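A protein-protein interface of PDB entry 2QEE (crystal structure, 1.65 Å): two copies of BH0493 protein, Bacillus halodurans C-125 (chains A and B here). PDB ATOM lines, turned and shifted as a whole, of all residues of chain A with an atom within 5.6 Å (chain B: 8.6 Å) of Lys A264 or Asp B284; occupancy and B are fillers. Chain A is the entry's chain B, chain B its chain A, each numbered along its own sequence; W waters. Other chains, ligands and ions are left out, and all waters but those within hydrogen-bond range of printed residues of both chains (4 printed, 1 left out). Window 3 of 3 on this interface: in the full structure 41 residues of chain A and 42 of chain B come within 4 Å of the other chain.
The side-chain amino group (NZ) of Lys A264 lies within salt-bridge range of the side-chain carboxylate (OD1) of Asp B284. OE1 of Glu B287 lies within salt-bridge range of NZ of Lys A264 (2.8 Å). O of Val A267 lies within hydrogen-bond range of NH1 of Arg B291, 2.9 Å away. NZ of Lys B317 lies within hydrogen-bond range of O of Asp A276 (2.7 Å).
The side-chain hydroxyl (OG) of Ser B282 sits at hydrogen-bond distance from the backbone NH (N) of Asp B284 (3.0 Å). SD of Met B283 sits at hydrogen-bond distance from ND2 of Asn B307, at 3.8 Å. The side-chain amide nitrogen (ND2) of Asn B307 lies within hydrogen-bond range of the side-chain carboxylate (OE2) of Glu B310, 2.8 Å away. The backbone carbonyl oxygen (O) of Lys A264 sits at hydrogen-bond distance from the backbone NH (N) of Phe A277 (2.8 Å). OD2 of Asp A276 lies within salt-bridge range of NZ of Lys A265. N of Val A267 lies within hydrogen-bond range of O of Gly A275, 2.8 Å away.
Among the printed residues, merely in contact across the chains: Phe A277 with Glu B310 (3.4 Å), Val A267 with Glu B287 (3.4 Å), Val A267 with Phe B318 (3.4 Å), Phe A277 with Leu B314 (3.5 Å), Phe A277 with Val B313 (3.6 Å), Phe A277 with Glu B287 (3.8 Å), Gly A275 with Lys B317 (3.8 Å), Val A278 with Val B313 (3.9 Å), Phe A277 with Met B283 (3.9 Å) and Val A267 with Lys B317 (3.9 Å).
No residue of chain B comes within 4 Å of Val A263. Of chain B, only Asp B284 and Glu B287 come within 4 Å of Lys A264. Printed residues of chain B within 4 Å of Phe A277: Met B283 (3.9 Å), Glu B287 (3.8 Å), Glu B310 (3.4 Å), Val B313 (3.6 Å) and Leu B314 (3.5 Å). Leu A303 touches none of the printed residues of chain B. Ser B282 touches none of the printed residues of chain A. Of the printed residues of chain A, Met B283 touches Phe A277 (3.9 Å). Asp B284 touches just one residue of chain A: Lys A264. Printed residues of chain A within 4 Å of Glu B310: Phe A277 (3.4 Å). Of the printed residues of chain A, Leu B314 touches Phe A277 (3.5 Å). The nearest residue of chain B that does not touch Lys A264 is Arg B291 (6.0 Å). The nearest printed residue of chain A that does not touch Asp B284 is Phe A277 (6.1 Å).
Hydrophobic or aromatic side chains of chain B within 4 Å of the printed part of chain A: Met B283, Val B313, Leu B314 and Phe B318. Of the 14 printed residues of chain A, 6 touch a printed residue of chain B. Among the printed residues, Asp or Glu carboxylates within 4 Å of a Lys or Arg side-chain nitrogen of the other chain: Lys A264 with Asp B284 and Lys A264 with Glu B287.
No position is printed for both chains. Of the 14 pairs that touch across the chains among the printed residues, none has its exchanged pair printed and touching as well.
Water W3 lies within hydrogen-bond range of O of Val A278 (2.6 Å) and OE1 of Glu B310 (2.8 Å). Water W2 lies within hydrogen-bond range of the side-chain carboxylate of Asp B284 (2.6 Å) and the side-chain amino group of Lys A264 (2.9 Å). Water W1 lies within hydrogen-bond range of O of Arg A266 (2.7 Å) and NH1 of Arg B291 (3.4 Å). Water W4 lies within hydrogen-bond range of the side-chain carboxylate of Glu B287, the side-chain carboxylate of Asp B284 and the side-chain amino group of Lys A264.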
ATOM      1  N   PRO A 227       2.075  -4.619   5.972  1.00  0.00           N
ATOM      2  CA  PRO A 227       1.925  -3.792   4.771  1.00  0.00           C
ATOM      3  C   PRO A 227       1.395  -2.404   5.081  1.00  0.00           C
ATOM      4  O   PRO A 227       0.975  -2.147   6.180  1.00  0.00           O
ATOM      5  CB  PRO A 227       0.845  -4.540   3.961  1.00  0.00           C
ATOM      6  CG  PRO A 227      -0.063  -5.125   5.077  1.00  0.00           C
ATOM      7  CD  PRO A 227       0.961  -5.600   6.101  1.00  0.00           C
ATOM      8  N   PRO A 228       1.446  -1.491   4.091  1.00  0.00           N
ATOM      9  CA  PRO A 228       0.987  -0.118   4.334  1.00  0.00           C
ATOM     10  C   PRO A 228      -0.484  -0.071   4.715  1.00  0.00           C
ATOM     11  O   PRO A 228      -0.927   0.876   5.351  1.00  0.00           O
ATOM     12  CB  PRO A 228       1.194   0.573   2.978  1.00  0.00           C
ATOM     13  CG  PRO A 228       2.315  -0.250   2.322  1.00  0.00           C
ATOM     14  CD  PRO A 228       2.043  -1.681   2.768  1.00  0.00           C
ATOM     15  N   GLY A 262       5.036  -1.047   6.695  1.00  0.00           N
ATOM     16  CA  GLY A 262       5.112  -0.230   5.475  1.00  0.00           C
ATOM     17  C   GLY A 262       5.673  -0.951   4.250  1.00  0.00           C
ATOM     18  O   GLY A 262       5.793  -0.334   3.183  1.00  0.00           O
ATOM     19  N   VAL A 263       6.003  -2.251   4.362  1.00  0.00           N
ATOM     20  CA  VAL A 263       6.591  -2.993   3.252  1.00  0.00           C
ATOM     21  C   VAL A 263       5.472  -3.594   2.387  1.00  0.00           C
ATOM     22  O   VAL A 263       4.524  -4.210   2.919  1.00  0.00           O
ATOM     23  CB  VAL A 263       7.598  -4.112   3.708  1.00  0.00           C
ATOM     24  CG1 VAL A 263       6.895  -5.105   4.582  1.00  0.00           C
ATOM     25  CG2 VAL A 263       8.173  -4.770   2.481  1.00  0.00           C
ATOM     26  N   LYS A 264       5.552  -3.286   1.086  1.00  0.00           N
ATOM     27  CA  LYS A 264       4.656  -3.847   0.066  1.00  0.00           C
ATOM     28  C   LYS A 264       5.442  -4.962  -0.646  1.00  0.00           C
ATOM     29  O   LYS A 264       6.354  -4.707  -1.443  1.00  0.00           O
ATOM     30  CB  LYS A 264       4.186  -2.739  -0.914  1.00  0.00           C
ATOM     31  CG  LYS A 264       2.950  -3.170  -1.746  1.00  0.00           C
ATOM     32  CD  LYS A 264       2.504  -2.108  -2.780  1.00  0.00           C
ATOM     33  CE  LYS A 264       1.592  -2.766  -3.819  1.00  0.00           C
ATOM     34  NZ  LYS A 264       0.770  -1.786  -4.577  1.00  0.00           N
ATOM     35  N   LYS A 265       5.069  -6.214  -0.345  1.00  0.00           N
ATOM     36  CA  LYS A 265       5.858  -7.380  -0.772  1.00  0.00           C
ATOM     37  C   LYS A 265       5.746  -7.675  -2.271  1.00  0.00           C
ATOM     38  O   LYS A 265       4.656  -7.590  -2.856  1.00  0.00           O
ATOM     39  CB  LYS A 265       5.430  -8.630   0.023  1.00  0.00           C
ATOM     40  CG  LYS A 265       5.739  -8.557   1.512  1.00  0.00           C
ATOM     41  CD  LYS A 265       7.202  -8.464   1.831  1.00  0.00           C
ATOM     42  CE  LYS A 265       7.908  -9.801   1.640  1.00  0.00           C
ATOM     43  NZ  LYS A 265       9.369  -9.620   1.921  1.00  0.00           N
ATOM     44  N   ARG A 266       6.899  -7.943  -2.873  1.00  0.00           N
ATOM     45  CA  ARG A 266       6.974  -8.529  -4.214  1.00  0.00           C
ATOM     46  C   ARG A 266       6.207  -7.756  -5.278  1.00  0.00           C
ATOM     47  O   ARG A 266       5.437  -8.340  -6.064  1.00  0.00           O
ATOM     48  CB  ARG A 266       6.516 -10.009  -4.184  1.00  0.00           C
ATOM     49  CG  ARG A 266       7.510 -10.921  -3.401  1.00  0.00           C
ATOM     50  CD  ARG A 266       8.985 -10.555  -3.701  1.00  0.00           C
ATOM     51  NE  ARG A 266       9.978 -11.438  -3.046  1.00  0.00           N
ATOM     52  CZ  ARG A 266      10.395 -11.330  -1.779  1.00  0.00           C
ATOM     53  NH1 ARG A 266       9.900 -10.392  -0.992  1.00  0.00           N
ATOM     54  NH2 ARG A 266      11.306 -12.178  -1.286  1.00  0.00           N
ATOM     55  N   VAL A 267       6.424  -6.445  -5.344  1.00  0.00           N
ATOM     56  CA  VAL A 267       5.896  -5.685  -6.489  1.00  0.00           C
ATOM     57  C   VAL A 267       6.621  -6.071  -7.797  1.00  0.00           C
ATOM     58  O   VAL A 267       6.095  -5.833  -8.887  1.00  0.00           O
ATOM     59  CB  VAL A 267       5.949  -4.115  -6.272  1.00  0.00           C
ATOM     60  CG1 VAL A 267       5.141  -3.733  -4.981  1.00  0.00           C
ATOM     61  CG2 VAL A 267       7.343  -3.611  -6.259  1.00  0.00           C
ATOM     62  N   GLY A 275      12.607  -7.135  -4.654  1.00  0.00           N
ATOM     63  CA  GLY A 275      11.381  -6.730  -5.350  1.00  0.00           C
ATOM     64  C   GLY A 275      10.317  -6.088  -4.455  1.00  0.00           C
ATOM     65  O   GLY A 275       9.183  -5.983  -4.868  1.00  0.00           O
ATOM     66  N   ASP A 276      10.683  -5.742  -3.219  1.00  0.00           N
ATOM     67  CA  ASP A 276       9.712  -5.224  -2.223  1.00  0.00           C
ATOM     68  C   ASP A 276       9.742  -3.701  -2.271  1.00  0.00           C
ATOM     69  O   ASP A 276      10.811  -3.103  -2.470  1.00  0.00           O
ATOM     70  CB  ASP A 276      10.110  -5.653  -0.820  1.00  0.00           C
ATOM     71  CG  ASP A 276       9.880  -7.147  -0.573  1.00  0.00           C
ATOM     72  OD1 ASP A 276       9.201  -7.850  -1.367  1.00  0.00           O
ATOM     73  OD2 ASP A 276      10.352  -7.604   0.471  1.00  0.00           O
ATOM     74  N   PHE A 277       8.550  -3.127  -2.094  1.00  0.00           N
ATOM     75  CA  PHE A 277       8.317  -1.684  -2.226  1.00  0.00           C
ATOM     76  C   PHE A 277       7.839  -1.142  -0.895  1.00  0.00           C
ATOM     77  O   PHE A 277       7.947  -1.820   0.173  1.00  0.00           O
ATOM     78  CB  PHE A 277       7.333  -1.517  -3.401  1.00  0.00           C
ATOM     79  CG  PHE A 277       7.078  -0.072  -3.856  1.00  0.00           C
ATOM     80  CD1 PHE A 277       8.122   0.847  -3.941  1.00  0.00           C
ATOM     81  CD2 PHE A 277       5.773   0.331  -4.198  1.00  0.00           C
ATOM     82  CE1 PHE A 277       7.867   2.211  -4.351  1.00  0.00           C
ATOM     83  CE2 PHE A 277       5.535   1.680  -4.635  1.00  0.00           C
ATOM     84  CZ  PHE A 277       6.607   2.592  -4.705  1.00  0.00           C
ATOM     85  N   VAL A 278       7.344   0.109  -0.920  1.00  0.00           N
ATOM     86  CA  VAL A 278       6.939   0.838   0.268  1.00  0.00           C
ATOM     87  C   VAL A 278       5.628   1.586   0.070  1.00  0.00           C
ATOM     88  O   VAL A 278       5.291   2.005  -1.050  1.00  0.00           O
ATOM     89  CB  VAL A 278       8.078   1.818   0.719  1.00  0.00           C
ATOM     90  CG1 VAL A 278       8.427   2.818  -0.405  1.00  0.00           C
ATOM     91  CG2 VAL A 278       7.754   2.515   2.045  1.00  0.00           C
ATOM     92  N   GLY A 279       4.925   1.790   1.166  1.00  0.00           N
ATOM     93  CA  GLY A 279       3.775   2.682   1.158  1.00  0.00           C
ATOM     94  C   GLY A 279       3.617   3.287   2.560  1.00  0.00           C
ATOM     95  O   GLY A 279       3.997   2.688   3.601  1.00  0.00           O
ATOM     96  N   LEU A 303       8.454   2.147   7.335  1.00  0.00           N
ATOM     97  CA  LEU A 303       9.277   2.175   6.123  1.00  0.00           C
ATOM     98  C   LEU A 303       9.123   3.453   5.303  1.00  0.00           C
ATOM     99  O   LEU A 303      10.103   3.853   4.611  1.00  0.00           O
ATOM    100  CB  LEU A 303       8.908   0.991   5.196  1.00  0.00           C
ATOM    101  CG  LEU A 303       9.943   0.624   4.112  1.00  0.00           C
ATOM    102  CD1 LEU A 303      11.437   0.381   4.579  1.00  0.00           C
ATOM    103  CD2 LEU A 303       9.403  -0.623   3.335  1.00  0.00           C
ATOM    104  N   PHE B 230      -4.584  10.199 -10.514  1.00  0.00           N
ATOM    105  CA  PHE B 230      -4.200   9.294 -11.591  1.00  0.00           C
ATOM    106  C   PHE B 230      -4.237   7.820 -11.165  1.00  0.00           C
ATOM    107  O   PHE B 230      -3.560   7.428 -10.212  1.00  0.00           O
ATOM    108  CB  PHE B 230      -2.831   9.604 -12.174  1.00  0.00           C
ATOM    109  CG  PHE B 230      -2.404   8.624 -13.228  1.00  0.00           C
ATOM    110  CD1 PHE B 230      -3.119   8.536 -14.442  1.00  0.00           C
ATOM    111  CD2 PHE B 230      -1.294   7.789 -13.040  1.00  0.00           C
ATOM    112  CE1 PHE B 230      -2.747   7.641 -15.450  1.00  0.00           C
ATOM    113  CE2 PHE B 230      -0.904   6.887 -14.055  1.00  0.00           C
ATOM    114  CZ  PHE B 230      -1.643   6.812 -15.261  1.00  0.00           C
ATOM    115  N   SER B 231      -4.969   6.996 -11.921  1.00  0.00           N
ATOM    116  CA  SER B 231      -4.995   5.569 -11.652  1.00  0.00           C
ATOM    117  C   SER B 231      -4.932   4.770 -12.942  1.00  0.00           C
ATOM    118  O   SER B 231      -5.342   5.236 -14.012  1.00  0.00           O
ATOM    119  CB  SER B 231      -6.191   5.177 -10.750  1.00  0.00           C
ATOM    120  OG  SER B 231      -7.415   5.314 -11.415  1.00  0.00           O
ATOM    121  N   PHE B 232      -4.306   3.604 -12.855  1.00  0.00           N
ATOM    122  CA  PHE B 232      -4.189   2.703 -13.979  1.00  0.00           C
ATOM    123  C   PHE B 232      -4.034   1.285 -13.478  1.00  0.00           C
ATOM    124  O   PHE B 232      -3.226   1.024 -12.584  1.00  0.00           O
ATOM    125  CB  PHE B 232      -2.998   3.066 -14.885  1.00  0.00           C
ATOM    126  CG  PHE B 232      -2.968   2.277 -16.161  1.00  0.00           C
ATOM    127  CD1 PHE B 232      -2.363   1.016 -16.198  1.00  0.00           C
ATOM    128  CD2 PHE B 232      -3.623   2.751 -17.313  1.00  0.00           C
ATOM    129  CE1 PHE B 232      -2.371   0.235 -17.370  1.00  0.00           C
ATOM    130  CE2 PHE B 232      -3.621   1.983 -18.486  1.00  0.00           C
ATOM    131  CZ  PHE B 232      -3.017   0.720 -18.509  1.00  0.00           C
ATOM    132  N   PRO B 233      -4.817   0.328 -14.047  1.00  0.00           N
ATOM    133  CA  PRO B 233      -5.857   0.388 -15.109  1.00  0.00           C
ATOM    134  C   PRO B 233      -7.020   1.265 -14.708  1.00  0.00           C
ATOM    135  O   PRO B 233      -7.265   1.497 -13.527  1.00  0.00           O
ATOM    136  CB  PRO B 233      -6.336  -1.075 -15.199  1.00  0.00           C
ATOM    137  CG  PRO B 233      -5.195  -1.875 -14.723  1.00  0.00           C
ATOM    138  CD  PRO B 233      -4.646  -1.050 -13.555  1.00  0.00           C
ATOM    139  N   ILE B 261       3.318  13.684 -13.081  1.00  0.00           N
ATOM    140  CA  ILE B 261       2.130  13.363 -12.241  1.00  0.00           C
ATOM    141  C   ILE B 261       2.006  14.274 -11.019  1.00  0.00           C
ATOM    142  O   ILE B 261       3.010  14.530 -10.308  1.00  0.00           O
ATOM    143  CB  ILE B 261       2.179  11.873 -11.750  1.00  0.00           C
ATOM    144  CG1 ILE B 261       2.233  10.890 -12.930  1.00  0.00           C
ATOM    145  CG2 ILE B 261       1.017  11.510 -10.815  1.00  0.00           C
ATOM    146  CD1 ILE B 261       2.739   9.499 -12.554  1.00  0.00           C
ATOM    147  N   ALA B 281      -0.022  11.745  -5.203  1.00  0.00           N
ATOM    148  CA  ALA B 281      -0.669  10.708  -6.012  1.00  0.00           C
ATOM    149  C   ALA B 281      -0.420   9.324  -5.367  1.00  0.00           C
ATOM    150  O   ALA B 281       0.556   9.113  -4.627  1.00  0.00           O
ATOM    151  CB  ALA B 281      -0.119  10.712  -7.439  1.00  0.00           C
ATOM    152  N   SER B 282      -1.304   8.370  -5.672  1.00  0.00           N
ATOM    153  CA  SER B 282      -0.968   6.951  -5.452  1.00  0.00           C
ATOM    154  C   SER B 282       0.154   6.509  -6.411  1.00  0.00           C
ATOM    155  O   SER B 282       0.180   6.926  -7.600  1.00  0.00           O
ATOM    156  CB  SER B 282      -2.196   6.054  -5.674  1.00  0.00           C
ATOM    157  OG  SER B 282      -1.792   4.702  -5.433  1.00  0.00           O
ATOM    158  N   MET B 283       1.031   5.625  -5.923  1.00  0.00           N
ATOM    159  CA  MET B 283       2.069   5.044  -6.744  1.00  0.00           C
ATOM    160  C   MET B 283       1.513   3.815  -7.513  1.00  0.00           C
ATOM    161  O   MET B 283       2.201   3.284  -8.386  1.00  0.00           O
ATOM    162  CB  MET B 283       3.319   4.636  -5.913  1.00  0.00           C
ATOM    163  CG  MET B 283       3.988   5.828  -5.156  1.00  0.00           C
ATOM    164  SD  MET B 283       4.440   7.154  -6.317  1.00  0.00           S
ATOM    165  CE  MET B 283       5.742   6.406  -7.313  1.00  0.00           C
ATOM    166  N   ASP B 284       0.282   3.384  -7.199  1.00  0.00           N
ATOM    167  CA  ASP B 284      -0.216   2.062  -7.691  1.00  0.00           C
ATOM    168  C   ASP B 284      -0.220   1.980  -9.208  1.00  0.00           C
ATOM    169  O   ASP B 284       0.087   0.936  -9.792  1.00  0.00           O
ATOM    170  CB  ASP B 284      -1.637   1.760  -7.220  1.00  0.00           C
ATOM    171  CG  ASP B 284      -1.708   1.444  -5.717  1.00  0.00           C
ATOM    172  OD1 ASP B 284      -0.644   1.415  -5.048  1.00  0.00           O
ATOM    173  OD2 ASP B 284      -2.817   1.209  -5.200  1.00  0.00           O
ATOM    174  N   GLY B 285      -0.673   3.064  -9.836  1.00  0.00           N
ATOM    175  CA  GLY B 285      -0.824   3.051 -11.310  1.00  0.00           C
ATOM    176  C   GLY B 285       0.518   2.996 -11.998  1.00  0.00           C
ATOM    177  O   GLY B 285       0.715   2.290 -13.008  1.00  0.00           O
ATOM    178  N   VAL B 286       1.468   3.786 -11.497  1.00  0.00           N
ATOM    179  CA  VAL B 286       2.817   3.719 -12.036  1.00  0.00           C
ATOM    180  C   VAL B 286       3.454   2.356 -11.815  1.00  0.00           C
ATOM    181  O   VAL B 286       4.128   1.817 -12.702  1.00  0.00           O
ATOM    182  CB  VAL B 286       3.764   4.830 -11.478  1.00  0.00           C
ATOM    183  CG1 VAL B 286       5.060   4.845 -12.253  1.00  0.00           C
ATOM    184  CG2 VAL B 286       3.087   6.210 -11.591  1.00  0.00           C
ATOM    185  N   GLU B 287       3.297   1.815 -10.607  1.00  0.00           N
ATOM    186  CA  GLU B 287       3.800   0.479 -10.298  1.00  0.00           C
ATOM    187  C   GLU B 287       3.235  -0.574 -11.284  1.00  0.00           C
ATOM    188  O   GLU B 287       3.984  -1.430 -11.826  1.00  0.00           O
ATOM    189  CB  GLU B 287       3.428   0.150  -8.834  1.00  0.00           C
ATOM    190  CG  GLU B 287       3.935  -1.258  -8.360  1.00  0.00           C
ATOM    191  CD  GLU B 287       3.095  -1.725  -7.175  1.00  0.00           C
ATOM    192  OE1 GLU B 287       2.877  -0.892  -6.263  1.00  0.00           O
ATOM    193  OE2 GLU B 287       2.667  -2.910  -7.153  1.00  0.00           O
ATOM    194  N   HIS B 288       1.928  -0.487 -11.531  1.00  0.00           N
ATOM    195  CA  HIS B 288       1.264  -1.414 -12.464  1.00  0.00           C
ATOM    196  C   HIS B 288       1.858  -1.295 -13.865  1.00  0.00           C
ATOM    197  O   HIS B 288       2.230  -2.319 -14.438  1.00  0.00           O
ATOM    198  CB  HIS B 288      -0.224  -1.159 -12.502  1.00  0.00           C
ATOM    199  CG  HIS B 288      -0.966  -2.064 -13.430  1.00  0.00           C
ATOM    200  ND1 HIS B 288      -1.716  -3.132 -12.977  1.00  0.00           N
ATOM    201  CD2 HIS B 288      -1.064  -2.073 -14.787  1.00  0.00           C
ATOM    202  CE1 HIS B 288      -2.261  -3.749 -14.015  1.00  0.00           C
ATOM    203  NE2 HIS B 288      -1.883  -3.127 -15.123  1.00  0.00           N
ATOM    204  N   LEU B 289       1.958  -0.063 -14.411  1.00  0.00           N
ATOM    205  CA  LEU B 289       2.557   0.129 -15.752  1.00  0.00           C
ATOM    206  C   LEU B 289       3.948  -0.478 -15.850  1.00  0.00           C
ATOM    207  O   LEU B 289       4.265  -1.186 -16.815  1.00  0.00           O
ATOM    208  CB  LEU B 289       2.617   1.612 -16.123  1.00  0.00           C
ATOM    209  CG  LEU B 289       1.250   2.251 -16.370  1.00  0.00           C
ATOM    210  CD1 LEU B 289       1.233   3.810 -16.179  1.00  0.00           C
ATOM    211  CD2 LEU B 289       0.872   1.813 -17.800  1.00  0.00           C
ATOM    212  N   LEU B 290       4.817  -0.179 -14.875  1.00  0.00           N
ATOM    213  CA  LEU B 290       6.197  -0.705 -14.911  1.00  0.00           C
ATOM    214  C   LEU B 290       6.267  -2.225 -14.894  1.00  0.00           C
ATOM    215  O   LEU B 290       7.079  -2.804 -15.636  1.00  0.00           O
ATOM    216  CB  LEU B 290       7.045  -0.112 -13.771  1.00  0.00           C
ATOM    217  CG  LEU B 290       7.211   1.411 -13.843  1.00  0.00           C
ATOM    218  CD1 LEU B 290       7.744   1.870 -12.452  1.00  0.00           C
ATOM    219  CD2 LEU B 290       8.227   1.773 -14.919  1.00  0.00           C
ATOM    220  N   ARG B 291       5.489  -2.850 -14.000  1.00  0.00           N
ATOM    221  CA  ARG B 291       5.500  -4.293 -13.852  1.00  0.00           C
ATOM    222  C   ARG B 291       4.892  -4.956 -15.093  1.00  0.00           C
ATOM    223  O   ARG B 291       5.435  -5.957 -15.585  1.00  0.00           O
ATOM    224  CB  ARG B 291       4.724  -4.718 -12.612  1.00  0.00           C
ATOM    225  CG  ARG B 291       4.588  -6.259 -12.446  1.00  0.00           C
ATOM    226  CD  ARG B 291       3.935  -6.682 -11.150  1.00  0.00           C
ATOM    227  NE  ARG B 291       2.690  -5.976 -10.976  1.00  0.00           N
ATOM    228  CZ  ARG B 291       2.483  -5.055 -10.035  1.00  0.00           C
ATOM    229  NH1 ARG B 291       3.460  -4.740  -9.160  1.00  0.00           N
ATOM    230  NH2 ARG B 291       1.306  -4.442  -9.971  1.00  0.00           N
ATOM    231  N   GLU B 292       3.749  -4.436 -15.539  1.00  0.00           N
ATOM    232  CA  GLU B 292       2.942  -5.189 -16.518  1.00  0.00           C
ATOM    233  C   GLU B 292       3.350  -4.901 -17.950  1.00  0.00           C
ATOM    234  O   GLU B 292       2.926  -5.609 -18.890  1.00  0.00           O
ATOM    235  CB  GLU B 292       1.452  -4.898 -16.332  1.00  0.00           C
ATOM    236  CG  GLU B 292       0.887  -5.209 -14.944  1.00  0.00           C
ATOM    237  CD  GLU B 292       1.098  -6.652 -14.449  1.00  0.00           C
ATOM    238  OE1 GLU B 292       1.379  -7.559 -15.261  1.00  0.00           O
ATOM    239  OE2 GLU B 292       0.950  -6.896 -13.228  1.00  0.00           O
ATOM    240  N   MET B 302       7.294  13.753 -10.511  1.00  0.00           N
ATOM    241  CA  MET B 302       6.055  13.974  -9.769  1.00  0.00           C
ATOM    242  C   MET B 302       6.108  15.287  -9.033  1.00  0.00           C
ATOM    243  O   MET B 302       7.202  15.803  -8.720  1.00  0.00           O
ATOM    244  CB  MET B 302       5.792  12.836  -8.743  1.00  0.00           C
ATOM    245  CG  MET B 302       5.743  11.451  -9.440  1.00  0.00           C
ATOM    246  SD  MET B 302       5.383  10.058  -8.346  1.00  0.00           S
ATOM    247  CE  MET B 302       3.643  10.307  -8.179  1.00  0.00           C
ATOM    248  N   ASN B 307       5.620  12.588  -2.593  1.00  0.00           N
ATOM    249  CA  ASN B 307       5.874  11.435  -3.545  1.00  0.00           C
ATOM    250  C   ASN B 307       7.323  11.103  -3.824  1.00  0.00           C
ATOM    251  O   ASN B 307       7.621  10.046  -4.372  1.00  0.00           O
ATOM    252  CB  ASN B 307       5.149  11.651  -4.903  1.00  0.00           C
ATOM    253  CG  ASN B 307       3.656  11.304  -4.875  1.00  0.00           C
ATOM    254  OD1 ASN B 307       2.863  12.097  -5.404  1.00  0.00           O
ATOM    255  ND2 ASN B 307       3.254  10.112  -4.316  1.00  0.00           N
ATOM    256  N   GLU B 310       9.265   7.763  -2.169  1.00  0.00           N
ATOM    257  CA  GLU B 310       8.723   6.518  -2.765  1.00  0.00           C
ATOM    258  C   GLU B 310       8.933   6.395  -4.285  1.00  0.00           C
ATOM    259  O   GLU B 310       9.143   5.303  -4.781  1.00  0.00           O
ATOM    260  CB  GLU B 310       7.290   6.312  -2.322  1.00  0.00           C
ATOM    261  CG  GLU B 310       6.348   7.370  -2.837  1.00  0.00           C
ATOM    262  CD  GLU B 310       4.980   7.304  -2.165  1.00  0.00           C
ATOM    263  OE1 GLU B 310       4.753   6.537  -1.190  1.00  0.00           O
ATOM    264  OE2 GLU B 310       4.103   8.047  -2.617  1.00  0.00           O
ATOM    265  N   VAL B 313      12.298   4.874  -4.487  1.00  0.00           N
ATOM    266  CA  VAL B 313      12.238   3.438  -4.184  1.00  0.00           C
ATOM    267  C   VAL B 313      11.686   2.664  -5.377  1.00  0.00           C
ATOM    268  O   VAL B 313      12.149   1.571  -5.687  1.00  0.00           O
ATOM    269  CB  VAL B 313      11.454   3.174  -2.905  1.00  0.00           C
ATOM    270  CG1 VAL B 313      11.412   1.632  -2.625  1.00  0.00           C
ATOM    271  CG2 VAL B 313      12.129   3.933  -1.738  1.00  0.00           C
ATOM    272  N   LEU B 314      10.734   3.244  -6.080  1.00  0.00           N
ATOM    273  CA  LEU B 314      10.099   2.492  -7.145  1.00  0.00           C
ATOM    274  C   LEU B 314      11.127   2.350  -8.256  1.00  0.00           C
ATOM    275  O   LEU B 314      11.155   1.316  -8.926  1.00  0.00           O
ATOM    276  CB  LEU B 314       8.863   3.257  -7.595  1.00  0.00           C
ATOM    277  CG  LEU B 314       8.040   2.561  -8.693  1.00  0.00           C
ATOM    278  CD1 LEU B 314       7.491   1.201  -8.203  1.00  0.00           C
ATOM    279  CD2 LEU B 314       6.923   3.537  -9.132  1.00  0.00           C
ATOM    280  N   LYS B 317      13.132  -0.584  -7.962  1.00  0.00           N
ATOM    281  CA  LYS B 317      12.438  -1.826  -8.309  1.00  0.00           C
ATOM    282  C   LYS B 317      12.402  -2.133  -9.790  1.00  0.00           C
ATOM    283  O   LYS B 317      12.363  -3.311 -10.189  1.00  0.00           O
ATOM    284  CB  LYS B 317      10.991  -1.846  -7.848  1.00  0.00           C
ATOM    285  CG  LYS B 317      10.685  -1.562  -6.399  1.00  0.00           C
ATOM    286  CD  LYS B 317      11.311  -2.557  -5.471  1.00  0.00           C
ATOM    287  CE  LYS B 317      12.646  -2.008  -4.813  1.00  0.00           C
ATOM    288  NZ  LYS B 317      13.118  -3.029  -3.779  1.00  0.00           N
ATOM    289  N   PHE B 318      12.398  -1.075 -10.608  1.00  0.00           N
ATOM    290  CA  PHE B 318      12.098  -1.208 -12.045  1.00  0.00           C
ATOM    291  C   PHE B 318      13.133  -0.488 -12.930  1.00  0.00           C
ATOM    292  O   PHE B 318      13.202   0.748 -12.980  1.00  0.00           O
ATOM    293  CB  PHE B 318      10.645  -0.782 -12.338  1.00  0.00           C
ATOM    294  CG  PHE B 318       9.590  -1.641 -11.670  1.00  0.00           C
ATOM    295  CD1 PHE B 318       9.311  -2.929 -12.132  1.00  0.00           C
ATOM    296  CD2 PHE B 318       8.876  -1.167 -10.597  1.00  0.00           C
ATOM    297  CE1 PHE B 318       8.310  -3.712 -11.519  1.00  0.00           C
ATOM    298  CE2 PHE B 318       7.884  -1.934  -9.976  1.00  0.00           C
ATOM    299  CZ  PHE B 318       7.607  -3.216 -10.452  1.00  0.00           C
HETATM  300  O   HOH W   1       3.351  -7.867  -7.743  1.00  0.00           O
HETATM  301  O   HOH W   2      -0.317   0.190  -2.770  1.00  0.00           O
HETATM  302  O   HOH W   3       4.385   4.007  -2.349  1.00  0.00           O
HETATM  303  O   HOH W   4       2.128   1.407  -4.972  1.00  0.00           O
